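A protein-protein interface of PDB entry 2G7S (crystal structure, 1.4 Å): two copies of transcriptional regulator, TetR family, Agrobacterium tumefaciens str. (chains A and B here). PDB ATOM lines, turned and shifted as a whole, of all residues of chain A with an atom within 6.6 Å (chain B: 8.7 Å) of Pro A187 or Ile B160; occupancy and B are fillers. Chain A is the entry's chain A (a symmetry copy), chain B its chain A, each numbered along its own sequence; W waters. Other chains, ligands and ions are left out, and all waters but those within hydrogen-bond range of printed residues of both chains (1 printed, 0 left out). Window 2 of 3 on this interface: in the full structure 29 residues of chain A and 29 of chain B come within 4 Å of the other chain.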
ATOM      1  N   THR A 164      -8.912  -0.027 -15.466  1.00  0.00           N
ATOM      2  CA  THR A 164      -8.573  -0.030 -16.914  1.00  0.00           C
ATOM      3  C   THR A 164      -7.408  -0.966 -17.168  1.00  0.00           C
ATOM      4  O   THR A 164      -7.440  -1.720 -18.156  1.00  0.00           O
ATOM      5  CB  THR A 164      -8.245   1.403 -17.370  1.00  0.00           C
ATOM      6  OG1 THR A 164      -9.407   2.254 -17.051  1.00  0.00           O
ATOM      7  CG2 THR A 164      -8.038   1.426 -18.850  1.00  0.00           C
ATOM      8  N   PHE A 181      -3.061  -3.835 -24.862  1.00  0.00           N
ATOM      9  CA  PHE A 181      -2.909  -3.298 -23.510  1.00  0.00           C
ATOM     10  C   PHE A 181      -2.602  -1.804 -23.549  1.00  0.00           C
ATOM     11  O   PHE A 181      -3.281  -0.995 -22.852  1.00  0.00           O
ATOM     12  CB  PHE A 181      -1.815  -4.052 -22.743  1.00  0.00           C
ATOM     13  CG  PHE A 181      -1.661  -3.592 -21.308  1.00  0.00           C
ATOM     14  CD1 PHE A 181      -2.478  -4.085 -20.301  1.00  0.00           C
ATOM     15  CD2 PHE A 181      -0.718  -2.649 -20.982  1.00  0.00           C
ATOM     16  CE1 PHE A 181      -2.342  -3.614 -18.968  1.00  0.00           C
ATOM     17  CE2 PHE A 181      -0.575  -2.175 -19.687  1.00  0.00           C
ATOM     18  CZ  PHE A 181      -1.384  -2.656 -18.667  1.00  0.00           C
ATOM     19  N   GLY A 182      -1.665  -1.390 -24.408  1.00  0.00           N
ATOM     20  CA  GLY A 182      -1.379   0.023 -24.531  1.00  0.00           C
ATOM     21  C   GLY A 182      -2.512   0.817 -25.176  1.00  0.00           C
ATOM     22  O   GLY A 182      -2.796   1.968 -24.824  1.00  0.00           O
ATOM     23  N   ALA A 183      -3.181   0.195 -26.161  1.00  0.00           N
ATOM     24  CA  ALA A 183      -4.252   0.911 -26.853  1.00  0.00           C
ATOM     25  C   ALA A 183      -5.391   1.257 -25.908  1.00  0.00           C
ATOM     26  O   ALA A 183      -6.148   2.239 -26.143  1.00  0.00           O
ATOM     27  CB  ALA A 183      -4.807   0.047 -27.973  1.00  0.00           C
ATOM     28  N   ILE A 184      -5.555   0.467 -24.847  1.00  0.00           N
ATOM     29  CA  ILE A 184      -6.629   0.745 -23.903  1.00  0.00           C
ATOM     30  C   ILE A 184      -6.146   1.678 -22.780  1.00  0.00           C
ATOM     31  O   ILE A 184      -6.961   2.557 -22.348  1.00  0.00           O
ATOM     32  CB  ILE A 184      -7.165  -0.573 -23.312  1.00  0.00           C
ATOM     33  CG1 ILE A 184      -7.936  -1.312 -24.407  1.00  0.00           C
ATOM     34  CG2 ILE A 184      -8.029  -0.360 -22.064  1.00  0.00           C
ATOM     35  CD1 ILE A 184      -8.204  -2.759 -24.056  1.00  0.00           C
ATOM     36  N   THR A 185      -4.921   1.481 -22.277  1.00  0.00           N
ATOM     37  CA  THR A 185      -4.517   2.210 -21.087  1.00  0.00           C
ATOM     38  C   THR A 185      -3.883   3.586 -21.380  1.00  0.00           C
ATOM     39  O   THR A 185      -3.995   4.502 -20.544  1.00  0.00           O
ATOM     40  CB  THR A 185      -3.500   1.414 -20.271  1.00  0.00           C
ATOM     41  OG1 THR A 185      -2.382   1.039 -21.090  1.00  0.00           O
ATOM     42  CG2 THR A 185      -4.122   0.149 -19.657  1.00  0.00           C
ATOM     43  N   ARG A 186      -3.252   3.719 -22.545  1.00  0.00           N
ATOM     44  CA  ARG A 186      -2.460   4.934 -22.781  1.00  0.00           C
ATOM     45  C   ARG A 186      -3.352   6.173 -23.022  1.00  0.00           C
ATOM     46  O   ARG A 186      -2.935   7.301 -22.725  1.00  0.00           O
ATOM     47  CB  ARG A 186      -1.413   4.687 -23.886  1.00  0.00           C
ATOM     48  CG  ARG A 186      -0.322   3.747 -23.292  1.00  0.00           C
ATOM     49  CD  ARG A 186       0.655   3.344 -24.410  1.00  0.00           C
ATOM     50  NE  ARG A 186       1.752   2.536 -23.882  1.00  0.00           N
ATOM     51  CZ  ARG A 186       2.748   3.075 -23.204  1.00  0.00           C
ATOM     52  NH1 ARG A 186       2.779   4.418 -22.965  1.00  0.00           N
ATOM     53  NH2 ARG A 186       3.747   2.281 -22.731  1.00  0.00           N
ATOM     54  N   PRO A 187      -4.512   6.035 -23.683  1.00  0.00           N
ATOM     55  CA  PRO A 187      -5.298   7.284 -23.895  1.00  0.00           C
ATOM     56  C   PRO A 187      -5.604   8.049 -22.593  1.00  0.00           C
ATOM     57  O   PRO A 187      -5.611   9.283 -22.601  1.00  0.00           O
ATOM     58  CB  PRO A 187      -6.538   6.808 -24.661  1.00  0.00           C
ATOM     59  CG  PRO A 187      -5.991   5.619 -25.476  1.00  0.00           C
ATOM     60  CD  PRO A 187      -5.055   4.908 -24.468  1.00  0.00           C
ATOM     61  N   MET A 188      -5.794   7.340 -21.469  1.00  0.00           N
ATOM     62  CA  MET A 188      -6.062   8.056 -20.200  1.00  0.00           C
ATOM     63  C   MET A 188      -4.873   8.918 -19.848  1.00  0.00           C
ATOM     64  O   MET A 188      -5.021  10.092 -19.454  1.00  0.00           O
ATOM     65  CB  MET A 188      -6.385   7.112 -19.032  1.00  0.00           C
ATOM     66  CG  MET A 188      -6.574   7.942 -17.716  1.00  0.00           C
ATOM     67  SD  MET A 188      -7.298   6.904 -16.299  1.00  0.00           S
ATOM     68  CE  MET A 188      -6.768   8.134 -14.766  1.00  0.00           C
ATOM     69  N   LEU A 189      -3.686   8.341 -20.004  1.00  0.00           N
ATOM     70  CA  LEU A 189      -2.436   9.016 -19.639  1.00  0.00           C
ATOM     71  C   LEU A 189      -2.305  10.281 -20.444  1.00  0.00           C
ATOM     72  O   LEU A 189      -1.932  11.343 -19.922  1.00  0.00           O
ATOM     73  CB  LEU A 189      -1.258   8.025 -19.898  1.00  0.00           C
ATOM     74  CG  LEU A 189      -0.717   7.352 -18.621  1.00  0.00           C
ATOM     75  CD1 LEU A 189       0.269   6.387 -19.167  1.00  0.00           C
ATOM     76  CD2 LEU A 189       0.075   8.293 -17.768  1.00  0.00           C
ATOM     77  N   GLU A 190      -2.629  10.217 -21.740  1.00  0.00           N
ATOM     78  CA  GLU A 190      -2.510  11.420 -22.548  1.00  0.00           C
ATOM     79  C   GLU A 190      -3.630  12.398 -22.234  1.00  0.00           C
ATOM     80  O   GLU A 190      -3.448  13.641 -22.222  1.00  0.00           O
ATOM     81  CB  GLU A 190      -2.444  11.007 -24.020  1.00  0.00           C
ATOM     82  CG  GLU A 190      -1.353   9.868 -24.328  1.00  0.00           C
ATOM     83  CD  GLU A 190       0.104  10.331 -24.004  1.00  0.00           C
ATOM     84  OE1 GLU A 190       0.433  11.502 -24.255  1.00  0.00           O
ATOM     85  OE2 GLU A 190       0.932   9.515 -23.484  1.00  0.00           O
ATOM     86  N   ARG A 191      -4.807  11.877 -21.866  1.00  0.00           N
ATOM     87  CA  ARG A 191      -5.844  12.818 -21.469  1.00  0.00           C
ATOM     88  C   ARG A 191      -5.344  13.706 -20.330  1.00  0.00           C
ATOM     89  O   ARG A 191      -5.346  14.954 -20.428  1.00  0.00           O
ATOM     90  CB  ARG A 191      -7.107  12.084 -21.078  1.00  0.00           C
ATOM     91  CG  ARG A 191      -8.273  12.932 -20.617  1.00  0.00           C
ATOM     92  CD  ARG A 191      -9.624  12.207 -20.766  1.00  0.00           C
ATOM     93  NE  ARG A 191      -9.551  10.742 -20.705  1.00  0.00           N
ATOM     94  CZ  ARG A 191      -9.545  10.048 -19.565  1.00  0.00           C
ATOM     95  NH1 ARG A 191      -9.583  10.697 -18.389  1.00  0.00           N
ATOM     96  NH2 ARG A 191      -9.466   8.717 -19.591  1.00  0.00           N
ATOM     97  N   ILE A 192      -4.893  13.051 -19.247  1.00  0.00           N
ATOM     98  CA  ILE A 192      -4.633  13.743 -17.947  1.00  0.00           C
ATOM     99  C   ILE A 192      -3.326  14.537 -17.971  1.00  0.00           C
ATOM    100  O   ILE A 192      -3.009  15.200 -16.991  1.00  0.00           O
ATOM    101  CB  ILE A 192      -4.640  12.764 -16.758  1.00  0.00           C
ATOM    102  CG1 ILE A 192      -3.432  11.869 -16.825  1.00  0.00           C
ATOM    103  CG2 ILE A 192      -6.044  12.062 -16.659  1.00  0.00           C
ATOM    104  CD1 ILE A 192      -3.306  10.871 -15.626  1.00  0.00           C
ATOM    105  N   SER B 132     -17.823  -5.687 -28.239  1.00  0.00           N
ATOM    106  CA  SER B 132     -17.061  -4.561 -28.791  1.00  0.00           C
ATOM    107  C   SER B 132     -17.769  -4.013 -30.039  1.00  0.00           C
ATOM    108  O   SER B 132     -17.868  -2.779 -30.222  1.00  0.00           O
ATOM    109  CB  SER B 132     -15.647  -5.028 -29.158  1.00  0.00           C
ATOM    110  OG  SER B 132     -14.943  -3.891 -29.667  1.00  0.00           O
ATOM    111  N   LEU B 135     -20.884  -1.944 -28.841  1.00  0.00           N
ATOM    112  CA  LEU B 135     -20.488  -0.646 -28.257  1.00  0.00           C
ATOM    113  C   LEU B 135     -19.956   0.291 -29.361  1.00  0.00           C
ATOM    114  O   LEU B 135     -20.180   1.502 -29.315  1.00  0.00           O
ATOM    115  CB  LEU B 135     -19.379  -0.889 -27.193  1.00  0.00           C
ATOM    116  CG  LEU B 135     -19.876  -1.601 -25.940  1.00  0.00           C
ATOM    117  CD1 LEU B 135     -18.649  -2.039 -25.154  1.00  0.00           C
ATOM    118  CD2 LEU B 135     -20.764  -0.655 -25.069  1.00  0.00           C
ATOM    119  N   THR B 136     -19.205  -0.261 -30.300  1.00  0.00           N
ATOM    120  CA  THR B 136     -18.653   0.563 -31.384  1.00  0.00           C
ATOM    121  C   THR B 136     -19.798   1.195 -32.164  1.00  0.00           C
ATOM    122  O   THR B 136     -19.766   2.385 -32.476  1.00  0.00           O
ATOM    123  CB  THR B 136     -17.754  -0.307 -32.343  1.00  0.00           C
ATOM    124  OG1 THR B 136     -16.610  -0.771 -31.617  1.00  0.00           O
ATOM    125  CG2 THR B 136     -17.279   0.498 -33.592  1.00  0.00           C
ATOM    126  N   LEU B 139     -21.445   3.964 -30.143  1.00  0.00           N
ATOM    127  CA  LEU B 139     -20.643   5.188 -30.146  1.00  0.00           C
ATOM    128  C   LEU B 139     -20.717   5.909 -31.532  1.00  0.00           C
ATOM    129  O   LEU B 139     -20.769   7.138 -31.602  1.00  0.00           O
ATOM    130  CB  LEU B 139     -19.187   4.836 -29.763  1.00  0.00           C
ATOM    131  CG  LEU B 139     -19.082   4.426 -28.277  1.00  0.00           C
ATOM    132  CD1 LEU B 139     -17.770   3.737 -28.111  1.00  0.00           C
ATOM    133  CD2 LEU B 139     -19.115   5.660 -27.374  1.00  0.00           C
ATOM    134  N   THR B 151     -12.344  11.298 -28.441  1.00  0.00           N
ATOM    135  CA  THR B 151     -10.945  11.350 -28.877  1.00  0.00           C
ATOM    136  C   THR B 151     -10.592   9.955 -29.402  1.00  0.00           C
ATOM    137  O   THR B 151     -10.793   8.987 -28.678  1.00  0.00           O
ATOM    138  CB  THR B 151     -10.083  11.717 -27.675  1.00  0.00           C
ATOM    139  OG1 THR B 151     -10.415  13.077 -27.291  1.00  0.00           O
ATOM    140  CG2 THR B 151      -8.610  11.597 -27.997  1.00  0.00           C
ATOM    141  N   GLY B 152     -10.093   9.851 -30.633  1.00  0.00           N
ATOM    142  CA  GLY B 152      -9.819   8.536 -31.209  1.00  0.00           C
ATOM    143  C   GLY B 152     -11.082   7.955 -31.822  1.00  0.00           C
ATOM    144  O   GLY B 152     -12.130   8.578 -31.817  1.00  0.00           O
ATOM    145  N   THR B 153     -10.953   6.759 -32.362  1.00  0.00           N
ATOM    146  CA  THR B 153     -12.076   6.206 -33.114  1.00  0.00           C
ATOM    147  C   THR B 153     -13.151   5.625 -32.206  1.00  0.00           C
ATOM    148  O   THR B 153     -12.920   5.332 -31.014  1.00  0.00           O
ATOM    149  CB  THR B 153     -11.559   5.055 -33.978  1.00  0.00           C
ATOM    150  OG1 THR B 153     -11.054   4.032 -33.152  1.00  0.00           O
ATOM    151  CG2 THR B 153     -10.436   5.566 -34.952  1.00  0.00           C
ATOM    152  N   ALA B 154     -14.316   5.374 -32.781  1.00  0.00           N
ATOM    153  CA  ALA B 154     -15.371   4.712 -32.008  1.00  0.00           C
ATOM    154  C   ALA B 154     -14.904   3.340 -31.546  1.00  0.00           C
ATOM    155  O   ALA B 154     -15.152   2.983 -30.381  1.00  0.00           O
ATOM    156  CB  ALA B 154     -16.619   4.564 -32.858  1.00  0.00           C
ATOM    157  N   ARG B 155     -14.254   2.565 -32.423  1.00  0.00           N
ATOM    158  CA  ARG B 155     -13.793   1.213 -31.959  1.00  0.00           C
ATOM    159  C   ARG B 155     -12.798   1.329 -30.811  1.00  0.00           C
ATOM    160  O   ARG B 155     -12.865   0.562 -29.826  1.00  0.00           O
ATOM    161  CB  ARG B 155     -13.114   0.484 -33.127  1.00  0.00           C
ATOM    162  CG  ARG B 155     -12.434  -0.828 -32.736  1.00  0.00           C
ATOM    163  CD  ARG B 155     -13.454  -1.855 -32.365  1.00  0.00           C
ATOM    164  NE  ARG B 155     -14.095  -2.358 -33.583  1.00  0.00           N
ATOM    165  CZ  ARG B 155     -15.007  -3.350 -33.611  1.00  0.00           C
ATOM    166  NH1 ARG B 155     -15.460  -3.914 -32.469  1.00  0.00           N
ATOM    167  NH2 ARG B 155     -15.473  -3.789 -34.774  1.00  0.00           N
ATOM    168  N   ALA B 156     -11.854   2.286 -30.883  1.00  0.00           N
ATOM    169  CA  ALA B 156     -10.894   2.374 -29.773  1.00  0.00           C
ATOM    170  C   ALA B 156     -11.587   2.756 -28.470  1.00  0.00           C
ATOM    171  O   ALA B 156     -11.264   2.228 -27.379  1.00  0.00           O
ATOM    172  CB  ALA B 156      -9.807   3.432 -30.075  1.00  0.00           C
ATOM    173  N   ASN B 157     -12.594   3.626 -28.571  1.00  0.00           N
ATOM    174  CA  ASN B 157     -13.366   3.966 -27.368  1.00  0.00           C
ATOM    175  C   ASN B 157     -14.215   2.797 -26.878  1.00  0.00           C
ATOM    176  O   ASN B 157     -14.404   2.653 -25.653  1.00  0.00           O
ATOM    177  CB  ASN B 157     -14.215   5.192 -27.628  1.00  0.00           C
ATOM    178  CG  ASN B 157     -13.375   6.463 -27.495  1.00  0.00           C
ATOM    179  OD1 ASN B 157     -13.211   6.985 -26.396  1.00  0.00           O
ATOM    180  ND2 ASN B 157     -12.809   6.930 -28.627  1.00  0.00           N
ATOM    181  N   ALA B 158     -14.763   2.016 -27.792  1.00  0.00           N
ATOM    182  CA  ALA B 158     -15.508   0.808 -27.378  1.00  0.00           C
ATOM    183  C   ALA B 158     -14.602  -0.161 -26.605  1.00  0.00           C
ATOM    184  O   ALA B 158     -15.011  -0.771 -25.618  1.00  0.00           O
ATOM    185  CB  ALA B 158     -16.030   0.077 -28.636  1.00  0.00           C
ATOM    186  N   GLU B 159     -13.383  -0.360 -27.106  1.00  0.00           N
ATOM    187  CA  GLU B 159     -12.457  -1.244 -26.434  1.00  0.00           C
ATOM    188  C   GLU B 159     -12.092  -0.729 -25.053  1.00  0.00           C
ATOM    189  O   GLU B 159     -11.995  -1.533 -24.083  1.00  0.00           O
ATOM    190  CB  GLU B 159     -11.208  -1.444 -27.299  1.00  0.00           C
ATOM    191  CG  GLU B 159     -11.420  -2.286 -28.552  1.00  0.00           C
ATOM    192  CD  GLU B 159     -11.612  -3.770 -28.230  1.00  0.00           C
ATOM    193  OE1 GLU B 159     -10.907  -4.282 -27.313  1.00  0.00           O
ATOM    194  OE2 GLU B 159     -12.390  -4.390 -28.957  1.00  0.00           O
ATOM    195  N   ILE B 160     -11.937   0.608 -24.906  1.00  0.00           N
ATOM    196  CA  ILE B 160     -11.703   1.175 -23.555  1.00  0.00           C
ATOM    197  C   ILE B 160     -12.936   0.973 -22.694  1.00  0.00           C
ATOM    198  O   ILE B 160     -12.817   0.596 -21.503  1.00  0.00           O
ATOM    199  CB  ILE B 160     -11.306   2.650 -23.702  1.00  0.00           C
ATOM    200  CG1 ILE B 160      -9.890   2.771 -24.327  1.00  0.00           C
ATOM    201  CG2 ILE B 160     -11.391   3.387 -22.356  1.00  0.00           C
ATOM    202  CD1 ILE B 160      -9.623   4.119 -24.975  1.00  0.00           C
ATOM    203  N   PHE B 161     -14.110   1.272 -23.218  1.00  0.00           N
ATOM    204  CA  PHE B 161     -15.276   1.150 -22.324  1.00  0.00           C
ATOM    205  C   PHE B 161     -15.519  -0.322 -21.924  1.00  0.00           C
ATOM    206  O   PHE B 161     -15.922  -0.610 -20.777  1.00  0.00           O
ATOM    207  CB  PHE B 161     -16.475   1.751 -23.050  1.00  0.00           C
ATOM    208  CG  PHE B 161     -17.725   1.764 -22.221  1.00  0.00           C
ATOM    209  CD1 PHE B 161     -17.867   2.698 -21.205  1.00  0.00           C
ATOM    210  CD2 PHE B 161     -18.773   0.878 -22.495  1.00  0.00           C
ATOM    211  CE1 PHE B 161     -19.033   2.691 -20.411  1.00  0.00           C
ATOM    212  CE2 PHE B 161     -19.942   0.888 -21.733  1.00  0.00           C
ATOM    213  CZ  PHE B 161     -20.070   1.832 -20.701  1.00  0.00           C
ATOM    214  N   MET B 162     -15.323  -1.264 -22.838  1.00  0.00           N
ATOM    215  CA  MET B 162     -15.512  -2.676 -22.461  1.00  0.00           C
ATOM    216  C   MET B 162     -14.484  -3.067 -21.421  1.00  0.00           C
ATOM    217  O   MET B 162     -14.826  -3.762 -20.421  1.00  0.00           O
ATOM    218  CB  MET B 162     -15.342  -3.559 -23.741  1.00  0.00           C
ATOM    219  CG  MET B 162     -15.537  -5.047 -23.377  1.00  0.00           C
ATOM    220  SD  MET B 162     -15.750  -6.168 -24.947  1.00  0.00           S
ATOM    221  CE  MET B 162     -13.926  -5.996 -25.631  1.00  0.00           C
ATOM    222  N   ALA B 163     -13.215  -2.666 -21.567  1.00  0.00           N
ATOM    223  CA  ALA B 163     -12.183  -3.015 -20.607  1.00  0.00           C
ATOM    224  C   ALA B 163     -12.510  -2.375 -19.243  1.00  0.00           C
ATOM    225  O   ALA B 163     -12.251  -2.950 -18.174  1.00  0.00           O
ATOM    226  CB  ALA B 163     -10.823  -2.567 -21.092  1.00  0.00           C
ATOM    227  N   THR B 164     -13.018  -1.142 -19.270  1.00  0.00           N
ATOM    228  CA  THR B 164     -13.376  -0.451 -18.003  1.00  0.00           C
ATOM    229  C   THR B 164     -14.493  -1.201 -17.306  1.00  0.00           C
ATOM    230  O   THR B 164     -14.436  -1.369 -16.075  1.00  0.00           O
ATOM    231  CB  THR B 164     -13.785   1.002 -18.306  1.00  0.00           C
ATOM    232  OG1 THR B 164     -12.665   1.646 -19.018  1.00  0.00           O
ATOM    233  CG2 THR B 164     -14.013   1.738 -17.025  1.00  0.00           C
ATOM    234  N   VAL B 165     -15.504  -1.661 -18.041  1.00  0.00           N
ATOM    235  CA  VAL B 165     -16.604  -2.452 -17.467  1.00  0.00           C
ATOM    236  C   VAL B 165     -16.037  -3.733 -16.835  1.00  0.00           C
ATOM    237  O   VAL B 165     -16.428  -4.075 -15.701  1.00  0.00           O
ATOM    238  CB  VAL B 165     -17.657  -2.741 -18.582  1.00  0.00           C
ATOM    239  CG1 VAL B 165     -18.582  -3.839 -18.235  1.00  0.00           C
ATOM    240  CG2 VAL B 165     -18.450  -1.437 -18.932  1.00  0.00           C
ATOM    241  N   HIS B 166     -15.201  -4.461 -17.600  1.00  0.00           N
ATOM    242  CA  HIS B 166     -14.706  -5.718 -17.050  1.00  0.00           C
ATOM    243  C   HIS B 166     -13.784  -5.455 -15.837  1.00  0.00           C
ATOM    244  O   HIS B 166     -13.831  -6.222 -14.840  1.00  0.00           O
ATOM    245  CB  HIS B 166     -13.954  -6.447 -18.116  1.00  0.00           C
ATOM    246  CG  HIS B 166     -14.851  -6.941 -19.196  1.00  0.00           C
ATOM    247  ND1 HIS B 166     -14.376  -7.253 -20.455  1.00  0.00           N
ATOM    248  CD2 HIS B 166     -16.181  -7.208 -19.209  1.00  0.00           C
ATOM    249  CE1 HIS B 166     -15.398  -7.699 -21.211  1.00  0.00           C
ATOM    250  NE2 HIS B 166     -16.513  -7.671 -20.477  1.00  0.00           N
ATOM    251  N   GLY B 167     -13.000  -4.372 -15.881  1.00  0.00           N
ATOM    252  CA  GLY B 167     -12.140  -4.086 -14.759  1.00  0.00           C
ATOM    253  C   GLY B 167     -12.984  -3.616 -13.575  1.00  0.00           C
ATOM    254  O   GLY B 167     -12.566  -3.811 -12.404  1.00  0.00           O
ATOM    255  N   ALA B 168     -14.091  -2.903 -13.820  1.00  0.00           N
ATOM    256  CA  ALA B 168     -14.939  -2.415 -12.730  1.00  0.00           C
ATOM    257  C   ALA B 168     -15.679  -3.578 -12.043  1.00  0.00           C
ATOM    258  O   ALA B 168     -15.841  -3.558 -10.811  1.00  0.00           O
ATOM    259  CB  ALA B 168     -15.941  -1.406 -13.294  1.00  0.00           C
ATOM    260  N   ILE B 184     -16.525   3.722 -11.298  1.00  0.00           N
ATOM    261  CA  ILE B 184     -15.454   3.556 -12.271  1.00  0.00           C
ATOM    262  C   ILE B 184     -15.969   3.790 -13.701  1.00  0.00           C
ATOM    263  O   ILE B 184     -15.196   4.385 -14.521  1.00  0.00           O
ATOM    264  CB  ILE B 184     -14.842   2.148 -12.145  1.00  0.00           C
ATOM    265  CG1 ILE B 184     -14.048   2.084 -10.840  1.00  0.00           C
ATOM    266  CG2 ILE B 184     -13.972   1.765 -13.348  1.00  0.00           C
ATOM    267  CD1 ILE B 184     -13.700   0.667 -10.438  1.00  0.00           C
ATOM    268  N   THR B 185     -17.176   3.307 -14.025  1.00  0.00           N
ATOM    269  CA  THR B 185     -17.601   3.335 -15.414  1.00  0.00           C
ATOM    270  C   THR B 185     -18.310   4.642 -15.826  1.00  0.00           C
ATOM    271  O   THR B 185     -18.234   5.033 -17.006  1.00  0.00           O
ATOM    272  CB  THR B 185     -18.563   2.189 -15.720  1.00  0.00           C
ATOM    273  OG1 THR B 185     -19.671   2.207 -14.807  1.00  0.00           O
ATOM    274  CG2 THR B 185     -17.867   0.820 -15.641  1.00  0.00           C
ATOM    275  N   MET B 188     -16.600   8.049 -17.620  1.00  0.00           N
ATOM    276  CA  MET B 188     -16.352   8.062 -19.081  1.00  0.00           C
ATOM    277  C   MET B 188     -17.579   8.576 -19.795  1.00  0.00           C
ATOM    278  O   MET B 188     -17.487   9.411 -20.717  1.00  0.00           O
ATOM    279  CB  MET B 188     -15.964   6.684 -19.638  1.00  0.00           C
ATOM    280  CG  MET B 188     -15.800   6.769 -21.195  1.00  0.00           C
ATOM    281  SD  MET B 188     -15.004   5.208 -21.928  1.00  0.00           S
ATOM    282  CE  MET B 188     -15.576   5.496 -23.861  1.00  0.00           C
ATOM    283  N   ARG B 191     -17.828  12.137 -19.490  1.00  0.00           N
ATOM    284  CA  ARG B 191     -16.836  12.814 -20.313  1.00  0.00           C
ATOM    285  C   ARG B 191     -17.366  13.000 -21.735  1.00  0.00           C
ATOM    286  O   ARG B 191     -17.431  14.133 -22.262  1.00  0.00           O
ATOM    287  CB  ARG B 191     -15.531  12.050 -20.310  1.00  0.00           C
ATOM    288  CG  ARG B 191     -14.405  12.622 -21.145  1.00  0.00           C
ATOM    289  CD  ARG B 191     -13.020  12.135 -20.676  1.00  0.00           C
ATOM    290  NE  ARG B 191     -13.015  10.828 -20.009  1.00  0.00           N
ATOM    291  CZ  ARG B 191     -12.969   9.665 -20.661  1.00  0.00           C
ATOM    292  NH1 ARG B 191     -12.949   9.652 -22.005  1.00  0.00           N
ATOM    293  NH2 ARG B 191     -12.979   8.516 -19.983  1.00  0.00           N
ATOM    294  N   ILE B 192     -17.767  11.875 -22.349  1.00  0.00           N
ATOM    295  CA  ILE B 192     -18.045  11.825 -23.818  1.00  0.00           C
ATOM    296  C   ILE B 192     -19.392  12.458 -24.169  1.00  0.00           C
ATOM    297  O   ILE B 192     -19.730  12.536 -25.344  1.00  0.00           O
ATOM    298  CB  ILE B 192     -17.971  10.389 -24.372  1.00  0.00           C
ATOM    299  CG1 ILE B 192     -19.131   9.581 -23.857  1.00  0.00           C
ATOM    300  CG2 ILE B 192     -16.531   9.803 -24.133  1.00  0.00           C
ATOM    301  CD1 ILE B 192     -19.188   8.117 -24.409  1.00  0.00           C
HETATM  302  O   HOH W   1      -8.605   1.176 -27.355  1.00  0.00           O
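Thr B164 touches its own counterpart, Thr A164. Arg B191 touches its own counterpart, Arg A191. Positions printed for both chains: 164, 184, 185, 188, 191 and 192. Of the 6 pairs that touch across the chains among the printed residues, 2 have their exchanged pair printed and touching as well.
Of the 13 printed residues of chain A, 4 touch a printed residue of chain B. Printed residues of chain A that touch a printed residue of chain B: Thr A164, Ile A184, Pro A187 and Arg A191. Hydrophobic or aromatic side chains of chain A within 4 Å of the printed part of chain B: Ile A184 and Pro A187. Among the printed residues, 6 pairs touch across the chains.
OG of Ser B132 lies within hydrogen-bond range of OE2 of Glu B159 (2.7 Å). The side-chain hydroxyl of Thr B164 sits at hydrogen-bond distance from the backbone carbonyl oxygen of Ile B160, at 2.7 Å.
Water W1 bridges the backbone carbonyl oxygen of Ala B156 and the backbone carbonyl oxygen of Ala A183.
Of the printed residues of chain B, Ile A184 touches Glu B159, Ile B160 and Ala B163. Pro A187 touches one residue of chain B. Glu A190 touches none of the printed residues of chain B. Thr B153 touches none of the printed residues of chain A. Printed residues of chain A within 4 Å of Glu B159: Ile A184. Ile B160 touches just these residues of chain A: Ile A184 and Pro A187. Printed residues of chain A within 4 Å of Ala B163: Ile A184. Printed residues of chain A within 4 Å of Thr B164: Thr A164 (3.9 Å). Of the printed residues of chain A, Arg B191 touches Arg A191 (3.4 Å). The nearest residue of chain A that does not touch Ile B160 is Ala A183 (4.1 Å).
Thr A164 touches Thr B164 (OG1 to OG1, 3.9 Å). CD1 of Ile A184 touches O of Glu B159 (3.98 Å). Ile A184 touches Ile B160 (O to CG1, 3.5 Å). Ala B163 touches Ile A184. Pro A187 touches Ile B160 (CG to CD1, 3.96 Å). Arg A191 touches Arg B191.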
